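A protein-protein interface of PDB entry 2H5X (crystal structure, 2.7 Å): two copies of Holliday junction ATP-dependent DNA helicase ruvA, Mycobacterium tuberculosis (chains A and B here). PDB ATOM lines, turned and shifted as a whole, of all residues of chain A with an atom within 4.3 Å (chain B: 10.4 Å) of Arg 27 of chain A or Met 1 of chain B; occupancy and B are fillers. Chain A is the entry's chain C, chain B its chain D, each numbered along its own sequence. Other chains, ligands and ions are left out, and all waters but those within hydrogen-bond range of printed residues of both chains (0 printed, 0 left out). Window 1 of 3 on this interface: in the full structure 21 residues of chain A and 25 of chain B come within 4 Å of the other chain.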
ATOM      1  N   ASP A  15     -20.132 -12.106  17.320  1.00  0.00           N
ATOM      2  CA  ASP A  15     -21.008 -10.968  17.557  1.00  0.00           C
ATOM      3  C   ASP A  15     -20.436  -9.681  16.972  1.00  0.00           C
ATOM      4  O   ASP A  15     -20.928  -8.586  17.257  1.00  0.00           O
ATOM      5  CB  ASP A  15     -21.256 -10.799  19.058  1.00  0.00           C
ATOM      6  CG  ASP A  15     -20.006 -10.404  19.818  1.00  0.00           C
ATOM      7  OD1 ASP A  15     -18.905 -10.856  19.437  1.00  0.00           O
ATOM      8  OD2 ASP A  15     -20.126  -9.651  20.812  1.00  0.00           O
ATOM      9  N   HIS A  16     -19.403  -9.808  16.144  1.00  0.00           N
ATOM     10  CA  HIS A  16     -18.802  -8.627  15.538  1.00  0.00           C
ATOM     11  C   HIS A  16     -17.676  -8.965  14.569  1.00  0.00           C
ATOM     12  O   HIS A  16     -17.120 -10.060  14.594  1.00  0.00           O
ATOM     13  CB  HIS A  16     -18.247  -7.705  16.626  1.00  0.00           C
ATOM     14  CG  HIS A  16     -16.954  -8.184  17.205  1.00  0.00           C
ATOM     15  ND1 HIS A  16     -15.765  -8.129  16.511  1.00  0.00           N
ATOM     16  CD2 HIS A  16     -16.675  -8.786  18.384  1.00  0.00           C
ATOM     17  CE1 HIS A  16     -14.807  -8.677  17.237  1.00  0.00           C
ATOM     18  NE2 HIS A  16     -15.333  -9.084  18.379  1.00  0.00           N
ATOM     19  N   VAL A  17     -17.332  -7.994  13.734  1.00  0.00           N
ATOM     20  CA  VAL A  17     -16.271  -8.144  12.755  1.00  0.00           C
ATOM     21  C   VAL A  17     -15.371  -6.901  12.829  1.00  0.00           C
ATOM     22  O   VAL A  17     -15.792  -5.844  13.319  1.00  0.00           O
ATOM     23  CB  VAL A  17     -16.868  -8.275  11.326  1.00  0.00           C
ATOM     24  CG1 VAL A  17     -17.558  -6.971  10.918  1.00  0.00           C
ATOM     25  CG2 VAL A  17     -15.771  -8.634  10.326  1.00  0.00           C
ATOM     26  N   GLY A  25      -8.545  -0.233  11.925  1.00  0.00           N
ATOM     27  CA  GLY A  25      -9.479  -1.335  12.035  1.00  0.00           C
ATOM     28  C   GLY A  25     -10.638  -1.007  12.949  1.00  0.00           C
ATOM     29  O   GLY A  25     -10.476  -0.828  14.163  1.00  0.00           O
ATOM     30  N   TYR A  26     -11.826  -0.924  12.366  1.00  0.00           N
ATOM     31  CA  TYR A  26     -13.000  -0.612  13.160  1.00  0.00           C
ATOM     32  C   TYR A  26     -13.769  -1.855  13.587  1.00  0.00           C
ATOM     33  O   TYR A  26     -14.004  -2.779  12.800  1.00  0.00           O
ATOM     34  CB  TYR A  26     -13.926   0.331  12.394  1.00  0.00           C
ATOM     35  CG  TYR A  26     -13.254   1.591  11.903  1.00  0.00           C
ATOM     36  CD1 TYR A  26     -12.439   1.570  10.773  1.00  0.00           C
ATOM     37  CD2 TYR A  26     -13.476   2.813  12.536  1.00  0.00           C
ATOM     38  CE1 TYR A  26     -11.873   2.733  10.278  1.00  0.00           C
ATOM     39  CE2 TYR A  26     -12.911   3.989  12.053  1.00  0.00           C
ATOM     40  CZ  TYR A  26     -12.115   3.946  10.921  1.00  0.00           C
ATOM     41  OH  TYR A  26     -11.569   5.113  10.420  1.00  0.00           O
ATOM     42  N   ARG A  27     -14.146  -1.883  14.855  1.00  0.00           N
ATOM     43  CA  ARG A  27     -14.901  -3.006  15.355  1.00  0.00           C
ATOM     44  C   ARG A  27     -16.342  -2.711  15.008  1.00  0.00           C
ATOM     45  O   ARG A  27     -16.856  -1.645  15.340  1.00  0.00           O
ATOM     46  CB  ARG A  27     -14.764  -3.135  16.866  1.00  0.00           C
ATOM     47  CG  ARG A  27     -15.573  -4.280  17.429  1.00  0.00           C
ATOM     48  CD  ARG A  27     -15.754  -4.116  18.901  1.00  0.00           C
ATOM     49  NE  ARG A  27     -16.751  -5.034  19.426  1.00  0.00           N
ATOM     50  CZ  ARG A  27     -16.473  -6.204  19.989  1.00  0.00           C
ATOM     51  NH1 ARG A  27     -15.217  -6.602  20.111  1.00  0.00           N
ATOM     52  NH2 ARG A  27     -17.459  -6.977  20.427  1.00  0.00           N
ATOM     53  N   VAL A  28     -16.991  -3.641  14.324  1.00  0.00           N
ATOM     54  CA  VAL A  28     -18.382  -3.442  13.973  1.00  0.00           C
ATOM     55  C   VAL A  28     -19.220  -4.597  14.491  1.00  0.00           C
ATOM     56  O   VAL A  28     -19.033  -5.741  14.081  1.00  0.00           O
ATOM     57  CB  VAL A  28     -18.554  -3.331  12.463  1.00  0.00           C
ATOM     58  CG1 VAL A  28     -19.998  -2.987  12.135  1.00  0.00           C
ATOM     59  CG2 VAL A  28     -17.602  -2.284  11.925  1.00  0.00           C
ATOM     60  N   ASN A  29     -20.129  -4.283  15.412  1.00  0.00           N
ATOM     61  CA  ASN A  29     -21.024  -5.273  16.007  1.00  0.00           C
ATOM     62  C   ASN A  29     -22.119  -5.605  15.014  1.00  0.00           C
ATOM     63  O   ASN A  29     -22.784  -4.716  14.482  1.00  0.00           O
ATOM     64  CB  ASN A  29     -21.612  -4.726  17.302  1.00  0.00           C
ATOM     65  CG  ASN A  29     -20.576  -4.619  18.393  1.00  0.00           C
ATOM     66  OD1 ASN A  29     -20.352  -5.565  19.156  1.00  0.00           O
ATOM     67  ND2 ASN A  29     -19.906  -3.478  18.454  1.00  0.00           N
ATOM     68  N   MET A  50     -23.635   4.569  13.955  1.00  0.00           N
ATOM     69  CA  MET A  50     -22.698   4.930  15.012  1.00  0.00           C
ATOM     70  C   MET A  50     -23.398   5.469  16.245  1.00  0.00           C
ATOM     71  O   MET A  50     -24.023   6.526  16.200  1.00  0.00           O
ATOM     72  CB  MET A  50     -21.688   5.965  14.494  1.00  0.00           C
ATOM     73  CG  MET A  50     -20.635   6.370  15.526  1.00  0.00           C
ATOM     74  SD  MET A  50     -19.370   7.444  14.841  1.00  0.00           S
ATOM     75  CE  MET A  50     -18.270   6.238  14.126  1.00  0.00           C
ATOM     76  N   MET A  57     -18.376   4.825  22.147  1.00  0.00           N
ATOM     77  CA  MET A  57     -18.539   5.195  20.748  1.00  0.00           C
ATOM     78  C   MET A  57     -18.510   3.865  20.008  1.00  0.00           C
ATOM     79  O   MET A  57     -17.440   3.325  19.725  1.00  0.00           O
ATOM     80  CB  MET A  57     -17.388   6.096  20.299  1.00  0.00           C
ATOM     81  CG  MET A  57     -17.666   6.872  19.027  1.00  0.00           C
ATOM     82  SD  MET A  57     -16.449   8.171  18.815  1.00  0.00           S
ATOM     83  CE  MET A  57     -16.931   9.296  20.142  1.00  0.00           C
ATOM     84  N   LEU A  59     -19.953   1.084  16.859  1.00  0.00           N
ATOM     85  CA  LEU A  59     -20.475   0.912  15.509  1.00  0.00           C
ATOM     86  C   LEU A  59     -21.352  -0.313  15.408  1.00  0.00           C
ATOM     87  O   LEU A  59     -21.168  -1.287  16.139  1.00  0.00           O
ATOM     88  CB  LEU A  59     -19.340   0.775  14.501  1.00  0.00           C
ATOM     89  CG  LEU A  59     -18.667   2.081  14.095  1.00  0.00           C
ATOM     90  CD1 LEU A  59     -17.416   1.778  13.247  1.00  0.00           C
ATOM     91  CD2 LEU A  59     -19.678   2.948  13.359  1.00  0.00           C
ATOM     92  N   MET B   1     -14.145   1.629  19.599  1.00  0.00           N
ATOM     93  CA  MET B   1     -14.520   1.632  18.158  1.00  0.00           C
ATOM     94  C   MET B   1     -13.296   1.310  17.320  1.00  0.00           C
ATOM     95  O   MET B   1     -13.344   0.438  16.462  1.00  0.00           O
ATOM     96  CB  MET B   1     -15.076   2.994  17.774  1.00  0.00           C
ATOM     97  CG  MET B   1     -15.547   3.078  16.358  1.00  0.00           C
ATOM     98  SD  MET B   1     -16.318   4.659  16.073  1.00  0.00           S
ATOM     99  CE  MET B   1     -14.951   5.642  15.477  1.00  0.00           C
ATOM    100  N   ILE B   2     -12.195   2.014  17.559  1.00  0.00           N
ATOM    101  CA  ILE B   2     -10.974   1.729  16.818  1.00  0.00           C
ATOM    102  C   ILE B   2     -10.346   0.489  17.452  1.00  0.00           C
ATOM    103  O   ILE B   2      -9.888   0.522  18.592  1.00  0.00           O
ATOM    104  CB  ILE B   2      -9.975   2.906  16.871  1.00  0.00           C
ATOM    105  CG1 ILE B   2     -10.472   4.051  15.979  1.00  0.00           C
ATOM    106  CG2 ILE B   2      -8.595   2.431  16.423  1.00  0.00           C
ATOM    107  CD1 ILE B   2      -9.521   5.228  15.882  1.00  0.00           C
ATOM    108  N   ALA B   3     -10.341  -0.609  16.704  1.00  0.00           N
ATOM    109  CA  ALA B   3      -9.809  -1.853  17.208  1.00  0.00           C
ATOM    110  C   ALA B   3      -8.336  -2.056  16.865  1.00  0.00           C
ATOM    111  O   ALA B   3      -7.675  -2.924  17.428  1.00  0.00           O
ATOM    112  CB  ALA B   3     -10.635  -2.995  16.677  1.00  0.00           C
ATOM    113  N   SER B   4      -7.810  -1.269  15.937  1.00  0.00           N
ATOM    114  CA  SER B   4      -6.403  -1.413  15.587  1.00  0.00           C
ATOM    115  C   SER B   4      -5.907  -0.281  14.687  1.00  0.00           C
ATOM    116  O   SER B   4      -6.687   0.393  14.012  1.00  0.00           O
ATOM    117  CB  SER B   4      -6.147  -2.772  14.905  1.00  0.00           C
ATOM    118  OG  SER B   4      -6.489  -2.745  13.526  1.00  0.00           O
ATOM    119  N   VAL B   5      -4.592  -0.084  14.699  1.00  0.00           N
ATOM    120  CA  VAL B   5      -3.939   0.940  13.899  1.00  0.00           C
ATOM    121  C   VAL B   5      -2.697   0.350  13.210  1.00  0.00           C
ATOM    122  O   VAL B   5      -1.829  -0.221  13.864  1.00  0.00           O
ATOM    123  CB  VAL B   5      -3.536   2.144  14.781  1.00  0.00           C
ATOM    124  CG1 VAL B   5      -2.812   3.185  13.949  1.00  0.00           C
ATOM    125  CG2 VAL B   5      -4.778   2.763  15.412  1.00  0.00           C
ATOM    126  N   TYR B  26      -1.798   8.552  15.131  1.00  0.00           N
ATOM    127  CA  TYR B  26      -2.509   8.260  16.369  1.00  0.00           C
ATOM    128  C   TYR B  26      -1.555   7.955  17.527  1.00  0.00           C
ATOM    129  O   TYR B  26      -0.582   7.217  17.368  1.00  0.00           O
ATOM    130  CB  TYR B  26      -3.449   7.066  16.167  1.00  0.00           C
ATOM    131  CG  TYR B  26      -4.490   7.256  15.094  1.00  0.00           C
ATOM    132  CD1 TYR B  26      -4.176   7.067  13.752  1.00  0.00           C
ATOM    133  CD2 TYR B  26      -5.793   7.645  15.420  1.00  0.00           C
ATOM    134  CE1 TYR B  26      -5.130   7.262  12.754  1.00  0.00           C
ATOM    135  CE2 TYR B  26      -6.756   7.848  14.430  1.00  0.00           C
ATOM    136  CZ  TYR B  26      -6.417   7.653  13.101  1.00  0.00           C
ATOM    137  OH  TYR B  26      -7.353   7.864  12.112  1.00  0.00           O
ATOM    138  N   LEU B  46      -0.910  -2.217  15.918  1.00  0.00           N
ATOM    139  CA  LEU B  46      -1.172  -2.577  17.305  1.00  0.00           C
ATOM    140  C   LEU B  46      -2.647  -2.798  17.568  1.00  0.00           C
ATOM    141  O   LEU B  46      -3.486  -2.009  17.138  1.00  0.00           O
ATOM    142  CB  LEU B  46      -0.669  -1.495  18.264  1.00  0.00           C
ATOM    143  CG  LEU B  46       0.820  -1.384  18.590  1.00  0.00           C
ATOM    144  CD1 LEU B  46       0.998  -0.404  19.749  1.00  0.00           C
ATOM    145  CD2 LEU B  46       1.376  -2.743  18.962  1.00  0.00           C
ATOM    146  N   ILE B  47      -2.971  -3.870  18.278  1.00  0.00           N
ATOM    147  CA  ILE B  47      -4.362  -4.127  18.604  1.00  0.00           C
ATOM    148  C   ILE B  47      -4.681  -3.142  19.728  1.00  0.00           C
ATOM    149  O   ILE B  47      -3.965  -3.083  20.733  1.00  0.00           O
ATOM    150  CB  ILE B  47      -4.553  -5.586  19.037  1.00  0.00           C
ATOM    151  CG1 ILE B  47      -3.997  -6.502  17.944  1.00  0.00           C
ATOM    152  CG2 ILE B  47      -6.037  -5.891  19.247  1.00  0.00           C
ATOM    153  CD1 ILE B  47      -4.419  -6.108  16.534  1.00  0.00           C
ATOM    154  N   THR B  48      -5.719  -2.339  19.526  1.00  0.00           N
ATOM    155  CA  THR B  48      -6.072  -1.314  20.497  1.00  0.00           C
ATOM    156  C   THR B  48      -7.412  -1.427  21.214  1.00  0.00           C
ATOM    157  O   THR B  48      -8.293  -2.202  20.839  1.00  0.00           O
ATOM    158  CB  THR B  48      -5.988   0.095  19.845  1.00  0.00           C
ATOM    159  OG1 THR B  48      -6.879   0.171  18.725  1.00  0.00           O
ATOM    160  CG2 THR B  48      -4.558   0.383  19.365  1.00  0.00           C
ATOM    161  N   ALA B  49      -7.527  -0.629  22.270  1.00  0.00           N
ATOM    162  CA  ALA B  49      -8.711  -0.545  23.108  1.00  0.00           C
ATOM    163  C   ALA B  49      -8.969   0.950  23.234  1.00  0.00           C
ATOM    164  O   ALA B  49      -8.231   1.652  23.931  1.00  0.00           O
ATOM    165  CB  ALA B  49      -8.427  -1.155  24.483  1.00  0.00           C
ATOM    166  N   MET B  50      -9.997   1.433  22.544  1.00  0.00           N
ATOM    167  CA  MET B  50     -10.329   2.853  22.579  1.00  0.00           C
ATOM    168  C   MET B  50     -11.284   3.179  23.720  1.00  0.00           C
ATOM    169  O   MET B  50     -12.439   2.753  23.724  1.00  0.00           O
ATOM    170  CB  MET B  50     -10.934   3.296  21.238  1.00  0.00           C
ATOM    171  CG  MET B  50     -11.194   4.793  21.144  1.00  0.00           C
ATOM    172  SD  MET B  50     -11.659   5.338  19.487  1.00  0.00           S
ATOM    173  CE  MET B  50     -13.446   5.453  19.639  1.00  0.00           C
ATOM    174  N   ILE B  51     -10.788   3.942  24.688  1.00  0.00           N
ATOM    175  CA  ILE B  51     -11.578   4.327  25.850  1.00  0.00           C
ATOM    176  C   ILE B  51     -12.104   5.741  25.661  1.00  0.00           C
ATOM    177  O   ILE B  51     -11.331   6.696  25.569  1.00  0.00           O
ATOM    178  CB  ILE B  51     -10.725   4.288  27.139  1.00  0.00           C
ATOM    179  CG1 ILE B  51     -10.032   2.926  27.276  1.00  0.00           C
ATOM    180  CG2 ILE B  51     -11.592   4.586  28.348  1.00  0.00           C
ATOM    181  CD1 ILE B  51     -10.963   1.730  27.242  1.00  0.00           C
ATOM    182  N   VAL B  52     -13.423   5.862  25.591  1.00  0.00           N
ATOM    183  CA  VAL B  52     -14.064   7.159  25.413  1.00  0.00           C
ATOM    184  C   VAL B  52     -14.551   7.704  26.756  1.00  0.00           C
ATOM    185  O   VAL B  52     -15.188   6.995  27.528  1.00  0.00           O
ATOM    186  CB  VAL B  52     -15.265   7.047  24.437  1.00  0.00           C
ATOM    187  CG1 VAL B  52     -16.005   8.370  24.352  1.00  0.00           C
ATOM    188  CG2 VAL B  52     -14.774   6.643  23.059  1.00  0.00           C
ATOM    189  N   MET B  57     -10.390  10.787  24.841  1.00  0.00           N
ATOM    190  CA  MET B  57     -10.533   9.674  23.910  1.00  0.00           C
ATOM    191  C   MET B  57      -9.100   9.163  23.804  1.00  0.00           C
ATOM    192  O   MET B  57      -8.278   9.779  23.129  1.00  0.00           O
ATOM    193  CB  MET B  57     -11.024  10.173  22.549  1.00  0.00           C
ATOM    194  CG  MET B  57     -12.507   9.956  22.299  1.00  0.00           C
ATOM    195  SD  MET B  57     -12.999  10.535  20.665  1.00  0.00           S
ATOM    196  CE  MET B  57     -11.973   9.495  19.621  1.00  0.00           C
ATOM    197  N   THR B  58      -8.800   8.050  24.473  1.00  0.00           N
ATOM    198  CA  THR B  58      -7.439   7.552  24.467  1.00  0.00           C
ATOM    199  C   THR B  58      -7.336   6.157  23.913  1.00  0.00           C
ATOM    200  O   THR B  58      -8.230   5.339  24.118  1.00  0.00           O
ATOM    201  CB  THR B  58      -6.874   7.567  25.902  1.00  0.00           C
ATOM    202  OG1 THR B  58      -6.920   8.906  26.417  1.00  0.00           O
ATOM    203  CG2 THR B  58      -5.446   7.052  25.929  1.00  0.00           C
ATOM    204  N   LEU B  59      -6.247   5.889  23.199  1.00  0.00           N
ATOM    205  CA  LEU B  59      -6.014   4.569  22.633  1.00  0.00           C
ATOM    206  C   LEU B  59      -4.938   3.830  23.423  1.00  0.00           C
ATOM    207  O   LEU B  59      -3.959   4.436  23.839  1.00  0.00           O
ATOM    208  CB  LEU B  59      -5.542   4.678  21.190  1.00  0.00           C
ATOM    209  CG  LEU B  59      -6.561   5.007  20.117  1.00  0.00           C
ATOM    210  CD1 LEU B  59      -5.882   4.954  18.748  1.00  0.00           C
ATOM    211  CD2 LEU B  59      -7.703   4.012  20.200  1.00  0.00           C
ATOM    212  N   TYR B  60      -5.137   2.525  23.624  1.00  0.00           N
ATOM    213  CA  TYR B  60      -4.180   1.656  24.318  1.00  0.00           C
ATOM    214  C   TYR B  60      -3.914   0.485  23.376  1.00  0.00           C
ATOM    215  O   TYR B  60      -4.842  -0.235  23.000  1.00  0.00           O
ATOM    216  CB  TYR B  60      -4.766   1.159  25.634  1.00  0.00           C
ATOM    217  CG  TYR B  60      -5.080   2.283  26.593  1.00  0.00           C
ATOM    218  CD1 TYR B  60      -6.314   2.951  26.542  1.00  0.00           C
ATOM    219  CD2 TYR B  60      -4.127   2.720  27.518  1.00  0.00           C
ATOM    220  CE1 TYR B  60      -6.582   4.024  27.384  1.00  0.00           C
ATOM    221  CE2 TYR B  60      -4.388   3.796  28.366  1.00  0.00           C
ATOM    222  CZ  TYR B  60      -5.613   4.443  28.294  1.00  0.00           C
ATOM    223  OH  TYR B  60      -5.850   5.521  29.122  1.00  0.00           O
ATOM    224  N   GLY B  65      -4.815  -9.625  20.021  1.00  0.00           N
ATOM    225  CA  GLY B  65      -6.167  -9.448  20.506  1.00  0.00           C
ATOM    226  C   GLY B  65      -6.280  -9.933  21.934  1.00  0.00           C
ATOM    227  O   GLY B  65      -6.856  -9.273  22.803  1.00  0.00           O
ATOM    228  N   ARG B  68      -5.093  -7.454  24.423  1.00  0.00           N
ATOM    229  CA  ARG B  68      -5.957  -6.276  24.416  1.00  0.00           C
ATOM    230  C   ARG B  68      -7.258  -6.545  25.177  1.00  0.00           C
ATOM    231  O   ARG B  68      -7.837  -5.630  25.772  1.00  0.00           O
ATOM    232  CB  ARG B  68      -6.239  -5.841  22.962  1.00  0.00           C
ATOM    233  CG  ARG B  68      -7.075  -4.562  22.803  1.00  0.00           C
ATOM    234  CD  ARG B  68      -8.572  -4.833  22.984  1.00  0.00           C
ATOM    235  NE  ARG B  68      -9.034  -5.884  22.079  1.00  0.00           N
ATOM    236  CZ  ARG B  68      -9.173  -5.742  20.763  1.00  0.00           C
ATOM    237  NH1 ARG B  68      -8.896  -4.585  20.174  1.00  0.00           N
ATOM    238  NH2 ARG B  68      -9.572  -6.772  20.030  1.00  0.00           N
ATOM    239  N   ASP B  69      -7.700  -7.802  25.166  1.00  0.00           N
ATOM    240  CA  ASP B  69      -8.930  -8.191  25.854  1.00  0.00           C
ATOM    241  C   ASP B  69      -8.710  -8.275  27.365  1.00  0.00           C
ATOM    242  O   ASP B  69      -9.584  -7.891  28.150  1.00  0.00           O
ATOM    243  CB  ASP B  69      -9.442  -9.534  25.328  1.00  0.00           C
ATOM    244  CG  ASP B  69     -10.054  -9.431  23.929  1.00  0.00           C
ATOM    245  OD1 ASP B  69     -10.188  -8.306  23.392  1.00  0.00           O
ATOM    246  OD2 ASP B  69     -10.407 -10.492  23.369  1.00  0.00           O
ATOM    247  N   LEU B  72      -9.054  -4.842  28.858  1.00  0.00           N
ATOM    248  CA  LEU B  72     -10.418  -4.388  29.108  1.00  0.00           C
ATOM    249  C   LEU B  72     -11.027  -5.074  30.332  1.00  0.00           C
ATOM    250  O   LEU B  72     -11.788  -4.465  31.089  1.00  0.00           O
ATOM    251  CB  LEU B  72     -11.281  -4.647  27.871  1.00  0.00           C
ATOM    252  CG  LEU B  72     -10.938  -3.903  26.574  1.00  0.00           C
ATOM    253  CD1 LEU B  72     -11.767  -4.455  25.400  1.00  0.00           C
ATOM    254  CD2 LEU B  72     -11.206  -2.416  26.776  1.00  0.00           C
ATOM    255  N   GLY B 157     -24.826 -14.696  25.225  1.00  0.00           N
ATOM    256  CA  GLY B 157     -24.475 -13.304  25.032  1.00  0.00           C
ATOM    257  C   GLY B 157     -25.655 -12.516  24.490  1.00  0.00           C
ATOM    258  O   GLY B 157     -25.655 -11.283  24.505  1.00  0.00           O
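The backbone carbonyl oxygen of Gly 25 of chain A lies within hydrogen-bond range of the backbone NH of Ala 3 of chain B, 2.6 Å away.
O of Ser 4 of chain B lies within hydrogen-bond range of N of Gly 25 of chain A, 2.9 Å away.
The backbone NH (N) of Arg 27 of chain A lies within hydrogen-bond range of the backbone carbonyl oxygen (O) of Met 1 of chain B (2.9 Å).
The side-chain carboxylate (OD2) of Asp 15 of chain A lies within salt-bridge range of the guanidinium group (NH2) of Arg 27 of chain A, at 3.8 Å.
A ring nitrogen (NE2) of His 16 of chain A lies within hydrogen-bond range of the guanidinium group of Arg 27 of chain A, 3.0 Å away.
The backbone NH (N) of Asn 29 of chain A lies within hydrogen-bond range of the backbone carbonyl oxygen (O) of Leu 59 of chain A.
O of Ile 2 of chain B sits at hydrogen-bond distance from OG1 of Thr 48 of chain B, at 3.0 Å.
O of Ala 3 of chain B lies within hydrogen-bond range of N of Thr 48 of chain B, 2.9 Å away.
The guanidinium group (NH1) of Arg 68 of chain B lies within hydrogen-bond range of the backbone carbonyl oxygen (O) of Ala 3 of chain B (3.4 Å).
Among the printed residues, pairs that only touch across the chains: Met 57 of chain A with Met 1 of chain B (3.1 Å), Met 50 of chain A with Met 1 of chain B (3.2 Å), Tyr 26 of chain A with Met 1 of chain B (3.5 Å), Gly 25 of chain A with Ile 2 of chain B (3.5 Å), Met 57 of chain A with Val 52 of chain B (3.8 Å), Leu 59 of chain A with Met 1 of chain B (3.9 Å) and Gly 25 of chain A with Met 1 of chain B (3.9 Å).
Arg 27 of chain A touches just one residue of chain B: Met 1 (2.9 Å).
Of chain A, only Gly 25 (3.9 Å), Tyr 26 (3.5 Å), Arg 27 (2.9 Å), Met 50 (3.2 Å), Met 57 (3.1 Å) and Leu 59 (3.9 Å) come within 4 Å of Met 1 of chain B.
No residue of chain B comes within 4 Å of Val 28 of chain A.
Of chain B, only Met 1 and Val 52 come within 4 Å of Met 57 of chain A.
Printed residues of chain A within 4 Å of Val 52 of chain B: Met 57.
Of the printed residues of chain B, Met 50 of chain A touches Met 1.
The nearest residue of chain B that does not touch Arg 27 of chain A is Ala 3 of chain B (4.1 Å).
The nearest printed residue of chain A that does not touch Met 1 of chain B is Val 28 of chain A (5.9 Å).
Printed residues of chain A that touch a printed residue of chain B: Gly 25, Tyr 26, Arg 27, Met 50, Met 57 and Leu 59.
Hydrophobic or aromatic side chains of chain A within 4 Å of the printed part of chain B: Met 50, Met 57 and Leu 59.
Printed residues of chain B that touch a printed residue of chain A: Met 1, Ile 2, Ala 3, Ser 4 and Val 52.
Hydrophobic or aromatic side chains of chain B that line the printed part of chain A: Met 1, Ala 3 and Val 52.
Among the printed residues, no Asp or Glu carboxylate lies within 4 Å of a Lys or Arg side-chain nitrogen of the other chain.
4 positions are printed for both chains.
Of the 10 pairs that touch across the chains among the printed residues, none has its exchanged pair printed and touching as well.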
